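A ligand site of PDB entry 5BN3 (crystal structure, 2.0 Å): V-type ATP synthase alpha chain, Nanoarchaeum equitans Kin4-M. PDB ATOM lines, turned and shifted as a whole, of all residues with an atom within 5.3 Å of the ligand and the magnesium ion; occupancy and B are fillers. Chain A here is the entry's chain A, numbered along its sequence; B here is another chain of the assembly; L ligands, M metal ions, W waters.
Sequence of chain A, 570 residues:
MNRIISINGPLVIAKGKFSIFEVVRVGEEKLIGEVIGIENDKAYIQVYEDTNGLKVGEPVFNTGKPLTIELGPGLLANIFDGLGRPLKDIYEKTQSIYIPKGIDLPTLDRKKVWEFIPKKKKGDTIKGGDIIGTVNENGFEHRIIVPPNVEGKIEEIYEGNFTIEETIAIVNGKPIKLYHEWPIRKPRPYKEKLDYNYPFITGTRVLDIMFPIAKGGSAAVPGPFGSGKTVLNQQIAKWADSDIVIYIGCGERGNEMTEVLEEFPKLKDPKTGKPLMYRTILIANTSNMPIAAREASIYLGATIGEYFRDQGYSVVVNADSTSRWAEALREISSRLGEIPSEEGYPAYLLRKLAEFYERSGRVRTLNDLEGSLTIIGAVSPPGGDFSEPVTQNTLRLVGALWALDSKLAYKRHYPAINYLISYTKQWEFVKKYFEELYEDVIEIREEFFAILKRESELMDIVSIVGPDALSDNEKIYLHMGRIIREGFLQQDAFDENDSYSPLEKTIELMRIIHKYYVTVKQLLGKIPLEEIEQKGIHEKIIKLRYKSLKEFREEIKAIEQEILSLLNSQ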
ATOM      1  N   PRO A 224      -0.936  -8.184 -34.823  1.00  0.00           N
ATOM      2  CA  PRO A 224      -1.788  -7.991 -33.646  1.00  0.00           C
ATOM      3  C   PRO A 224      -1.102  -8.536 -32.399  1.00  0.00           C
ATOM      4  O   PRO A 224      -0.059  -9.185 -32.534  1.00  0.00           O
ATOM      5  CB  PRO A 224      -3.026  -8.825 -33.966  1.00  0.00           C
ATOM      6  CG  PRO A 224      -2.537  -9.873 -34.933  1.00  0.00           C
ATOM      7  CD  PRO A 224      -1.480  -9.184 -35.761  1.00  0.00           C
ATOM      8  N   PHE A 225      -1.657  -8.293 -31.217  1.00  0.00           N
ATOM      9  CA  PHE A 225      -1.032  -8.822 -30.003  1.00  0.00           C
ATOM     10  C   PHE A 225      -1.004 -10.348 -30.010  1.00  0.00           C
ATOM     11  O   PHE A 225      -1.970 -11.004 -30.404  1.00  0.00           O
ATOM     12  CB  PHE A 225      -1.671  -8.262 -28.723  1.00  0.00           C
ATOM     13  CG  PHE A 225      -3.066  -8.762 -28.446  1.00  0.00           C
ATOM     14  CD1 PHE A 225      -3.288  -9.968 -27.782  1.00  0.00           C
ATOM     15  CD2 PHE A 225      -4.174  -8.004 -28.802  1.00  0.00           C
ATOM     16  CE1 PHE A 225      -4.569 -10.416 -27.522  1.00  0.00           C
ATOM     17  CE2 PHE A 225      -5.456  -8.440 -28.547  1.00  0.00           C
ATOM     18  CZ  PHE A 225      -5.661  -9.643 -27.897  1.00  0.00           C
ATOM     19  N   GLY A 226       0.124 -10.925 -29.593  1.00  0.00           N
ATOM     20  CA  GLY A 226       0.273 -12.362 -29.530  1.00  0.00           C
ATOM     21  C   GLY A 226       0.657 -13.038 -30.835  1.00  0.00           C
ATOM     22  O   GLY A 226       0.718 -14.264 -30.908  1.00  0.00           O
ATOM     23  N   SER A 227       0.918 -12.242 -31.873  1.00  0.00           N
ATOM     24  CA  SER A 227       1.246 -12.807 -33.178  1.00  0.00           C
ATOM     25  C   SER A 227       2.726 -13.186 -33.316  1.00  0.00           C
ATOM     26  O   SER A 227       3.081 -13.981 -34.192  1.00  0.00           O
ATOM     27  CB  SER A 227       0.806 -11.879 -34.322  1.00  0.00           C
ATOM     28  OG  SER A 227       1.498 -10.645 -34.282  1.00  0.00           O
ATOM     29  N   GLY A 228       3.589 -12.622 -32.470  1.00  0.00           N
ATOM     30  CA  GLY A 228       4.964 -13.077 -32.413  1.00  0.00           C
ATOM     31  C   GLY A 228       6.071 -12.092 -32.752  1.00  0.00           C
ATOM     32  O   GLY A 228       7.193 -12.504 -33.030  1.00  0.00           O
ATOM     33  N   LYS A 229       5.760 -10.795 -32.728  1.00  0.00           N
ATOM     34  CA  LYS A 229       6.735  -9.743 -33.033  1.00  0.00           C
ATOM     35  C   LYS A 229       7.972  -9.813 -32.153  1.00  0.00           C
ATOM     36  O   LYS A 229       9.105  -9.766 -32.643  1.00  0.00           O
ATOM     37  CB  LYS A 229       6.124  -8.360 -32.843  1.00  0.00           C
ATOM     38  CG  LYS A 229       5.043  -7.939 -33.808  1.00  0.00           C
ATOM     39  CD  LYS A 229       4.522  -6.580 -33.377  1.00  0.00           C
ATOM     40  CE  LYS A 229       3.095  -6.658 -32.884  1.00  0.00           C
ATOM     41  NZ  LYS A 229       2.827  -7.664 -31.822  1.00  0.00           N
ATOM     42  N   THR A 230       7.745  -9.890 -30.848  1.00  0.00           N
ATOM     43  CA  THR A 230       8.822  -9.839 -29.866  1.00  0.00           C
ATOM     44  C   THR A 230       9.763 -11.037 -29.972  1.00  0.00           C
ATOM     45  O   THR A 230      10.981 -10.889 -29.952  1.00  0.00           O
ATOM     46  CB  THR A 230       8.270  -9.731 -28.432  1.00  0.00           C
ATOM     47  OG1 THR A 230       7.588  -8.475 -28.274  1.00  0.00           O
ATOM     48  CG2 THR A 230       9.390  -9.817 -27.414  1.00  0.00           C
ATOM     49  N   VAL A 231       9.195 -12.236 -30.096  1.00  0.00           N
ATOM     50  CA  VAL A 231       9.990 -13.441 -30.270  1.00  0.00           C
ATOM     51  C   VAL A 231      10.782 -13.379 -31.569  1.00  0.00           C
ATOM     52  O   VAL A 231      11.969 -13.733 -31.606  1.00  0.00           O
ATOM     53  CB  VAL A 231       9.105 -14.710 -30.244  1.00  0.00           C
ATOM     54  CG1 VAL A 231       9.910 -15.928 -30.667  1.00  0.00           C
ATOM     55  CG2 VAL A 231       8.542 -14.916 -28.847  1.00  0.00           C
ATOM     56  N   LEU A 232      10.142 -12.921 -32.641  1.00  0.00           N
ATOM     57  CA  LEU A 232      10.811 -12.811 -33.942  1.00  0.00           C
ATOM     58  C   LEU A 232      12.003 -11.867 -33.877  1.00  0.00           C
ATOM     59  O   LEU A 232      13.062 -12.184 -34.390  1.00  0.00           O
ATOM     60  CB  LEU A 232       9.832 -12.369 -35.026  1.00  0.00           C
ATOM     61  CG  LEU A 232      10.444 -12.336 -36.430  1.00  0.00           C
ATOM     62  CD1 LEU A 232      10.915 -13.717 -36.813  1.00  0.00           C
ATOM     63  CD2 LEU A 232       9.455 -11.815 -37.461  1.00  0.00           C
ATOM     64  N   GLN A 235      14.756 -13.461 -31.820  1.00  0.00           N
ATOM     65  CA  GLN A 235      15.418 -14.491 -32.629  1.00  0.00           C
ATOM     66  C   GLN A 235      16.440 -13.871 -33.561  1.00  0.00           C
ATOM     67  O   GLN A 235      17.533 -14.389 -33.737  1.00  0.00           O
ATOM     68  CB  GLN A 235      14.390 -15.279 -33.450  1.00  0.00           C
ATOM     69  CG  GLN A 235      13.597 -16.289 -32.643  1.00  0.00           C
ATOM     70  CD  GLN A 235      14.495 -17.301 -31.946  1.00  0.00           C
ATOM     71  OE1 GLN A 235      14.722 -17.215 -30.736  1.00  0.00           O
ATOM     72  NE2 GLN A 235      14.990 -18.265 -32.701  1.00  0.00           N
ATOM     73  N   GLU A 252       7.496  -1.542 -24.082  1.00  0.00           N
ATOM     74  CA  GLU A 252       6.985  -2.905 -23.937  1.00  0.00           C
ATOM     75  C   GLU A 252       7.193  -3.470 -22.529  1.00  0.00           C
ATOM     76  O   GLU A 252       7.418  -2.721 -21.587  1.00  0.00           O
ATOM     77  CB  GLU A 252       7.603  -3.829 -24.991  1.00  0.00           C
ATOM     78  CG  GLU A 252       7.173  -3.511 -26.417  1.00  0.00           C
ATOM     79  CD  GLU A 252       5.693  -3.705 -26.643  1.00  0.00           C
ATOM     80  OE1 GLU A 252       5.133  -4.704 -26.144  1.00  0.00           O
ATOM     81  OE2 GLU A 252       5.078  -2.853 -27.334  1.00  0.00           O
ATOM     82  N   ARG A 253       7.108  -4.801 -22.399  1.00  0.00           N
ATOM     83  CA  ARG A 253       7.128  -5.444 -21.083  1.00  0.00           C
ATOM     84  C   ARG A 253       8.516  -5.495 -20.439  1.00  0.00           C
ATOM     85  O   ARG A 253       9.522  -5.765 -21.110  1.00  0.00           O
ATOM     86  CB  ARG A 253       6.555  -6.869 -21.170  1.00  0.00           C
ATOM     87  CG  ARG A 253       5.110  -6.931 -21.660  1.00  0.00           C
ATOM     88  CD  ARG A 253       4.589  -8.355 -21.749  1.00  0.00           C
ATOM     89  NE  ARG A 253       3.256  -8.396 -22.361  1.00  0.00           N
ATOM     90  CZ  ARG A 253       3.040  -8.530 -23.666  1.00  0.00           C
ATOM     91  NH1 ARG A 253       4.062  -8.632 -24.499  1.00  0.00           N
ATOM     92  NH2 ARG A 253       1.801  -8.549 -24.143  1.00  0.00           N
ATOM     93  N   GLU A 256      10.376  -8.876 -20.673  1.00  0.00           N
ATOM     94  CA  GLU A 256      10.977  -9.228 -21.955  1.00  0.00           C
ATOM     95  C   GLU A 256      12.428  -8.748 -22.038  1.00  0.00           C
ATOM     96  O   GLU A 256      13.259  -9.370 -22.689  1.00  0.00           O
ATOM     97  CB  GLU A 256      10.138  -8.689 -23.120  1.00  0.00           C
ATOM     98  CG  GLU A 256       8.824  -9.442 -23.288  1.00  0.00           C
ATOM     99  CD  GLU A 256       7.758  -8.655 -24.006  1.00  0.00           C
ATOM    100  OE1 GLU A 256       8.010  -7.475 -24.348  1.00  0.00           O
ATOM    101  OE2 GLU A 256       6.661  -9.203 -24.232  1.00  0.00           O
ATOM    102  N   ASP A 320      11.225  -2.475 -30.707  1.00  0.00           N
ATOM    103  CA  ASP A 320       9.986  -3.136 -30.288  1.00  0.00           C
ATOM    104  C   ASP A 320       9.381  -2.366 -29.119  1.00  0.00           C
ATOM    105  O   ASP A 320       9.850  -2.503 -27.991  1.00  0.00           O
ATOM    106  CB  ASP A 320      10.322  -4.576 -29.874  1.00  0.00           C
ATOM    107  CG  ASP A 320       9.105  -5.368 -29.422  1.00  0.00           C
ATOM    108  OD1 ASP A 320       7.970  -5.013 -29.810  1.00  0.00           O
ATOM    109  OD2 ASP A 320       9.277  -6.366 -28.677  1.00  0.00           O
ATOM    110  N   LEU A 404       2.852 -10.267 -39.810  1.00  0.00           N
ATOM    111  CA  LEU A 404       2.430 -11.370 -38.962  1.00  0.00           C
ATOM    112  C   LEU A 404       0.915 -11.551 -39.024  1.00  0.00           C
ATOM    113  O   LEU A 404       0.159 -10.578 -39.124  1.00  0.00           O
ATOM    114  CB  LEU A 404       2.908 -11.166 -37.531  1.00  0.00           C
ATOM    115  CG  LEU A 404       4.436 -11.135 -37.386  1.00  0.00           C
ATOM    116  CD1 LEU A 404       4.853 -10.931 -35.950  1.00  0.00           C
ATOM    117  CD2 LEU A 404       5.024 -12.425 -37.926  1.00  0.00           C
ATOM    118  N   TYR A 414       4.354 -20.702 -36.133  1.00  0.00           N
ATOM    119  CA  TYR A 414       5.332 -19.645 -35.898  1.00  0.00           C
ATOM    120  C   TYR A 414       6.634 -19.923 -36.662  1.00  0.00           C
ATOM    121  O   TYR A 414       7.069 -21.071 -36.725  1.00  0.00           O
ATOM    122  CB  TYR A 414       5.665 -19.516 -34.409  1.00  0.00           C
ATOM    123  CG  TYR A 414       4.499 -19.352 -33.474  1.00  0.00           C
ATOM    124  CD1 TYR A 414       3.751 -18.178 -33.453  1.00  0.00           C
ATOM    125  CD2 TYR A 414       4.176 -20.347 -32.564  1.00  0.00           C
ATOM    126  CE1 TYR A 414       2.682 -18.031 -32.575  1.00  0.00           C
ATOM    127  CE2 TYR A 414       3.116 -20.210 -31.693  1.00  0.00           C
ATOM    128  CZ  TYR A 414       2.380 -19.050 -31.695  1.00  0.00           C
ATOM    129  OH  TYR A 414       1.332 -18.918 -30.818  1.00  0.00           O
ATOM    130  N   PRO A 415       7.248 -18.880 -37.234  1.00  0.00           N
ATOM    131  CA  PRO A 415       6.780 -17.488 -37.304  1.00  0.00           C
ATOM    132  C   PRO A 415       5.502 -17.346 -38.127  1.00  0.00           C
ATOM    133  O   PRO A 415       5.369 -17.965 -39.179  1.00  0.00           O
ATOM    134  CB  PRO A 415       7.929 -16.769 -38.039  1.00  0.00           C
ATOM    135  CG  PRO A 415       9.124 -17.629 -37.791  1.00  0.00           C
ATOM    136  CD  PRO A 415       8.596 -19.033 -37.798  1.00  0.00           C
ATOM    137  N   GLN A 491       9.246 -22.555 -37.569  1.00  0.00           N
ATOM    138  CA  GLN A 491      10.534 -22.667 -36.894  1.00  0.00           C
ATOM    139  C   GLN A 491      10.355 -22.391 -35.404  1.00  0.00           C
ATOM    140  O   GLN A 491       9.975 -21.292 -35.002  1.00  0.00           O
ATOM    141  CB  GLN A 491      11.546 -21.703 -37.517  1.00  0.00           C
ATOM    142  CG  GLN A 491      12.972 -21.873 -36.999  1.00  0.00           C
ATOM    143  CD  GLN A 491      14.001 -21.165 -37.856  1.00  0.00           C
ATOM    144  OE1 GLN A 491      13.727 -20.766 -38.985  1.00  0.00           O
ATOM    145  NE2 GLN A 491      15.205 -20.998 -37.319  1.00  0.00           N
ATOM    146  N   ASP A 492      10.631 -23.410 -34.583  1.00  0.00           N
ATOM    147  CA  ASP A 492      10.437 -23.323 -33.137  1.00  0.00           C
ATOM    148  C   ASP A 492      11.588 -22.558 -32.496  1.00  0.00           C
ATOM    149  O   ASP A 492      12.720 -23.031 -32.442  1.00  0.00           O
ATOM    150  CB  ASP A 492      10.336 -24.731 -32.548  1.00  0.00           C
ATOM    151  CG  ASP A 492       9.785 -24.731 -31.120  1.00  0.00           C
ATOM    152  OD1 ASP A 492       9.790 -23.665 -30.468  1.00  0.00           O
ATOM    153  OD2 ASP A 492       9.357 -25.797 -30.655  1.00  0.00           O
ATOM    154  N   ALA A 493      11.287 -21.366 -31.989  1.00  0.00           N
ATOM    155  CA  ALA A 493      12.292 -20.508 -31.367  1.00  0.00           C
ATOM    156  C   ALA A 493      12.826 -21.083 -30.060  1.00  0.00           C
ATOM    157  O   ALA A 493      13.883 -20.672 -29.582  1.00  0.00           O
ATOM    158  CB  ALA A 493      11.725 -19.131 -31.133  1.00  0.00           C
ATOM    159  N   PHE A 494      12.076 -22.014 -29.478  1.00  0.00           N
ATOM    160  CA  PHE A 494      12.424 -22.550 -28.173  1.00  0.00           C
ATOM    161  C   PHE A 494      12.738 -24.054 -28.209  1.00  0.00           C
ATOM    162  O   PHE A 494      12.610 -24.752 -27.203  1.00  0.00           O
ATOM    163  CB  PHE A 494      11.326 -22.227 -27.154  1.00  0.00           C
ATOM    164  CG  PHE A 494      10.923 -20.778 -27.156  1.00  0.00           C
ATOM    165  CD1 PHE A 494      11.827 -19.809 -26.763  1.00  0.00           C
ATOM    166  CD2 PHE A 494       9.666 -20.395 -27.579  1.00  0.00           C
ATOM    167  CE1 PHE A 494      11.478 -18.467 -26.775  1.00  0.00           C
ATOM    168  CE2 PHE A 494       9.307 -19.052 -27.588  1.00  0.00           C
ATOM    169  CZ  PHE A 494      10.213 -18.088 -27.186  1.00  0.00           C
ATOM    170  N   LEU B 324      -4.199 -17.510 -24.427  1.00  0.00           N
ATOM    171  CA  LEU B 324      -2.742 -17.518 -24.514  1.00  0.00           C
ATOM    172  C   LEU B 324      -2.113 -17.258 -23.151  1.00  0.00           C
ATOM    173  O   LEU B 324      -2.564 -16.400 -22.401  1.00  0.00           O
ATOM    174  CB  LEU B 324      -2.273 -16.459 -25.509  1.00  0.00           C
ATOM    175  CG  LEU B 324      -0.759 -16.191 -25.542  1.00  0.00           C
ATOM    176  CD1 LEU B 324      -0.023 -17.400 -26.057  1.00  0.00           C
ATOM    177  CD2 LEU B 324      -0.427 -14.957 -26.369  1.00  0.00           C
ATOM    178  N   SER B 325      -1.070 -18.018 -22.836  1.00  0.00           N
ATOM    179  CA  SER B 325      -0.188 -17.683 -21.731  1.00  0.00           C
ATOM    180  C   SER B 325       1.211 -17.543 -22.301  1.00  0.00           C
ATOM    181  O   SER B 325       1.810 -18.529 -22.728  1.00  0.00           O
ATOM    182  CB  SER B 325      -0.219 -18.774 -20.659  1.00  0.00           C
ATOM    183  OG  SER B 325       0.710 -18.494 -19.628  1.00  0.00           O
ATOM    184  N   ARG B 326       1.726 -16.310 -22.329  1.00  0.00           N
ATOM    185  CA  ARG B 326       3.007 -16.035 -22.974  1.00  0.00           C
ATOM    186  C   ARG B 326       4.197 -16.729 -22.321  1.00  0.00           C
ATOM    187  O   ARG B 326       5.123 -17.152 -23.013  1.00  0.00           O
ATOM    188  CB  ARG B 326       3.281 -14.520 -23.005  1.00  0.00           C
ATOM    189  CG  ARG B 326       2.557 -13.775 -24.109  1.00  0.00           C
ATOM    190  CD  ARG B 326       2.826 -12.291 -24.041  1.00  0.00           C
ATOM    191  NE  ARG B 326       1.709 -11.508 -24.576  1.00  0.00           N
ATOM    192  CZ  ARG B 326       1.587 -11.163 -25.852  1.00  0.00           C
ATOM    193  NH1 ARG B 326       2.505 -11.525 -26.729  1.00  0.00           N
ATOM    194  NH2 ARG B 326       0.537 -10.455 -26.248  1.00  0.00           N
ATOM    195  N   LEU B 327       4.160 -16.839 -21.002  1.00  0.00           N
ATOM    196  CA  LEU B 327       5.297 -17.356 -20.248  1.00  0.00           C
ATOM    197  C   LEU B 327       5.171 -18.854 -19.972  1.00  0.00           C
ATOM    198  O   LEU B 327       6.069 -19.443 -19.375  1.00  0.00           O
ATOM    199  CB  LEU B 327       5.474 -16.578 -18.947  1.00  0.00           C
ATOM    200  CG  LEU B 327       5.606 -15.062 -19.067  1.00  0.00           C
ATOM    201  CD1 LEU B 327       5.872 -14.426 -17.710  1.00  0.00           C
ATOM    202  CD2 LEU B 327       6.715 -14.712 -20.030  1.00  0.00           C
HETATM  203  P1  LIG L   1       3.741 -10.202 -29.719  1.00  0.00           P
HETATM  204  O1  LIG L   1       3.423 -10.067 -31.185  1.00  0.00           O
HETATM  205  O2  LIG L   1       5.065  -9.630 -29.299  1.00  0.00           O
HETATM  206  O3  LIG L   1       2.591  -9.839 -28.815  1.00  0.00           O
HETATM  207  P2  LIG L   1       5.118 -12.566 -28.819  1.00  0.00           P
HETATM  208  O4  LIG L   1       6.398 -12.335 -29.565  1.00  0.00           O
HETATM  209  O5  LIG L   1       5.052 -12.274 -27.340  1.00  0.00           O
HETATM  210  O6  LIG L   1       3.915 -11.803 -29.572  1.00  0.00           O
HETATM  211  O7  LIG L   1       4.694 -14.104 -29.046  1.00  0.00           O
HETATM  212  C1  LIG L   1       3.410 -14.560 -28.617  1.00  0.00           C
HETATM  213  C2  LIG L   1       3.463 -16.046 -28.300  1.00  0.00           C
HETATM  214  O8  LIG L   1       3.806 -16.792 -29.481  1.00  0.00           O
HETATM  215  C3  LIG L   1       4.525 -16.320 -27.257  1.00  0.00           C
HETATM  216  O9  LIG L   1       3.938 -17.050 -26.171  1.00  0.00           O
HETATM  217  C4  LIG L   1       5.566 -17.149 -27.962  1.00  0.00           C
HETATM  218  O10 LIG L   1       6.017 -18.228 -27.136  1.00  0.00           O
HETATM  219  C5  LIG L   1       4.889 -17.671 -29.214  1.00  0.00           C
HETATM  220  N1  LIG L   1       5.853 -17.677 -30.338  1.00  0.00           N
HETATM  221  C6  LIG L   1       6.078 -16.652 -31.196  1.00  0.00           C
HETATM  222  N2  LIG L   1       7.020 -16.981 -32.108  1.00  0.00           N
HETATM  223  C7  LIG L   1       7.420 -18.237 -31.838  1.00  0.00           C
HETATM  224  C8  LIG L   1       8.392 -19.193 -32.427  1.00  0.00           C
HETATM  225  N3  LIG L   1       9.143 -18.866 -33.503  1.00  0.00           N
HETATM  226  N4  LIG L   1       8.490 -20.416 -31.844  1.00  0.00           N
HETATM  227  C9  LIG L   1       7.748 -20.753 -30.774  1.00  0.00           C
HETATM  228  N5  LIG L   1       6.847 -19.940 -30.194  1.00  0.00           N
HETATM  229  C10 LIG L   1       6.645 -18.685 -30.677  1.00  0.00           C
HETATM  230 MG    MG M   1       5.591  -8.218 -27.878  1.00  0.00          MG
HETATM  231  O   HOH W   1       5.751  -9.839 -26.602  1.00  0.00           O
HETATM  232  O   HOH W   2       7.525 -15.129 -33.981  1.00  0.00           O
HETATM  233  O   HOH W   3      10.151 -16.392 -34.420  1.00  0.00           O
HETATM  234  O   HOH W   4       6.186  -6.929 -26.340  1.00  0.00           O
HETATM  235  O   HOH W   5       3.572  -7.880 -27.505  1.00  0.00           O
HETATM  236  O   HOH W   6       5.630  -6.522 -29.065  1.00  0.00           O
HETATM  237  O   HOH W   7      11.702 -18.828 -35.320  1.00  0.00           O
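N of Thr 230 lies within hydrogen-bond range of O4 of the ligand (3.1 Å).
The backbone NH (N) of Lys 229 is in hydrogen-bond range of an oxygen (O1) of the ligand, 2.9 Å away.
NZ of Lys 229 is in salt-bridge range of O1 of the ligand (2.6 Å).
An oxygen (O9) of the ligand sits at hydrogen-bond distance from the backbone carbonyl oxygen of Arg 326 of chain B, 3.4 Å away.
O3 of the ligand is in salt-bridge range of NH1 of Arg 326 of chain B, at 2.7 Å.
N of Gly 226 is in hydrogen-bond range of O3 of the ligand (2.8 Å).
The backbone NH (N) of Val 231 lies within hydrogen-bond range of an oxygen (O4) of the ligand (2.8 Å).
O1 of the ligand is in hydrogen-bond range of N of Gly 228 (2.9 Å).
The backbone NH (N) of Ala 493 sits at hydrogen-bond distance from a nitrogen (N4) of the ligand, at 3.0 Å.
The backbone carbonyl oxygen (O) of Gln 491 sits at hydrogen-bond distance from a nitrogen (N3) of the ligand (3.0 Å).
N of Ser 227 lies within hydrogen-bond range of O1 of the ligand (3.4 Å).
OD2 of Asp 320 lies close to OG1 of Thr 230 (2.7 Å).
NZ of Lys 229 sits at hydrogen-bond distance from O of Pro 224, at 3.3 Å.
N of Gln 491 lies within hydrogen-bond range of O of Tyr 414 (2.8 Å).
The backbone carbonyl oxygen (O) of Pro 224 sits at hydrogen-bond distance from the side-chain hydroxyl (OG) of Ser 227 (2.8 Å).
The backbone NH (N) of Phe 494 is in hydrogen-bond range of the side-chain carboxylate (OD1) of Asp 492, at 3.0 Å.
The guanidinium group of Arg 253 lies within salt-bridge range of the side-chain carboxylate of Glu 256, at 2.7 Å.
Residues that only touch the ligand: Pro 224 (3.8 Å), Phe 225 (3.8 Å), Tyr 414 (3.4 Å), Asp 492 (3.6 Å), Phe 494 (3.4 Å) and Leu 324 of chain B (3.98 Å).
Within 4 Å of the ligand: Pro 224, Phe 225, Gly 226, Ser 227, Gly 228, Lys 229, Thr 230, Val 231, Tyr 414, Gln 491, Asp 492, Ala 493, Phe 494, Leu 324 of chain B and Arg 326 of chain B.
The nearest printed residue that does not touch the ligand is Pro 415 (4.2 Å).
OE1 of Glu 252 touches the magnesium ion, at 3.9 Å.
NH1 of Arg 253 touches the magnesium ion, at 3.7 Å.
Glu 256 touches the magnesium ion (OE2 to MG, 3.9 Å).
The nearest printed residue that does not touch the magnesium ion is Asp 320 (4.2 Å).
The magnesium ion is bound by OG1 of Thr 230 (2.1 Å), water W1 (2.1 Å), O2 of the ligand (2.1 Å), water W6 (2.1 Å), water W5 (2.1 Å) and water W4 (2.1 Å).
The magnesium ion has six donor atoms within binding distance.
Water W6 lies within hydrogen-bond range of OD1 of Asp 320 (2.9 Å) and OE1 of Glu 252 (3.5 Å).
Water W5 bridges an oxygen (O3) of the ligand (2.6 Å) and the guanidinium group of Arg 253 (3.1 Å).
Water W1 lies within hydrogen-bond range of the side-chain carboxylate (OE2) of Glu 256 (2.6 Å), an oxygen (O5) of the ligand (2.6 Å) and the guanidinium group (NH1) of Arg 253 (3.0 Å).
Water W4 lies within hydrogen-bond range of the side-chain carboxylate (OE1) of Glu 252 (2.5 Å), the side-chain carboxylate (OE1) of Glu 256 (2.8 Å) and the guanidinium group (NH1) of Arg 253 (3.3 Å).
Water W2 bridges a nitrogen (N2) of the ligand (2.7 Å) and the backbone carbonyl oxygen (O) of Gly 228 (2.8 Å).
Water W7 lies within hydrogen-bond range of O of Gln 491 (3.0 Å) and N3 of the ligand (3.1 Å).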
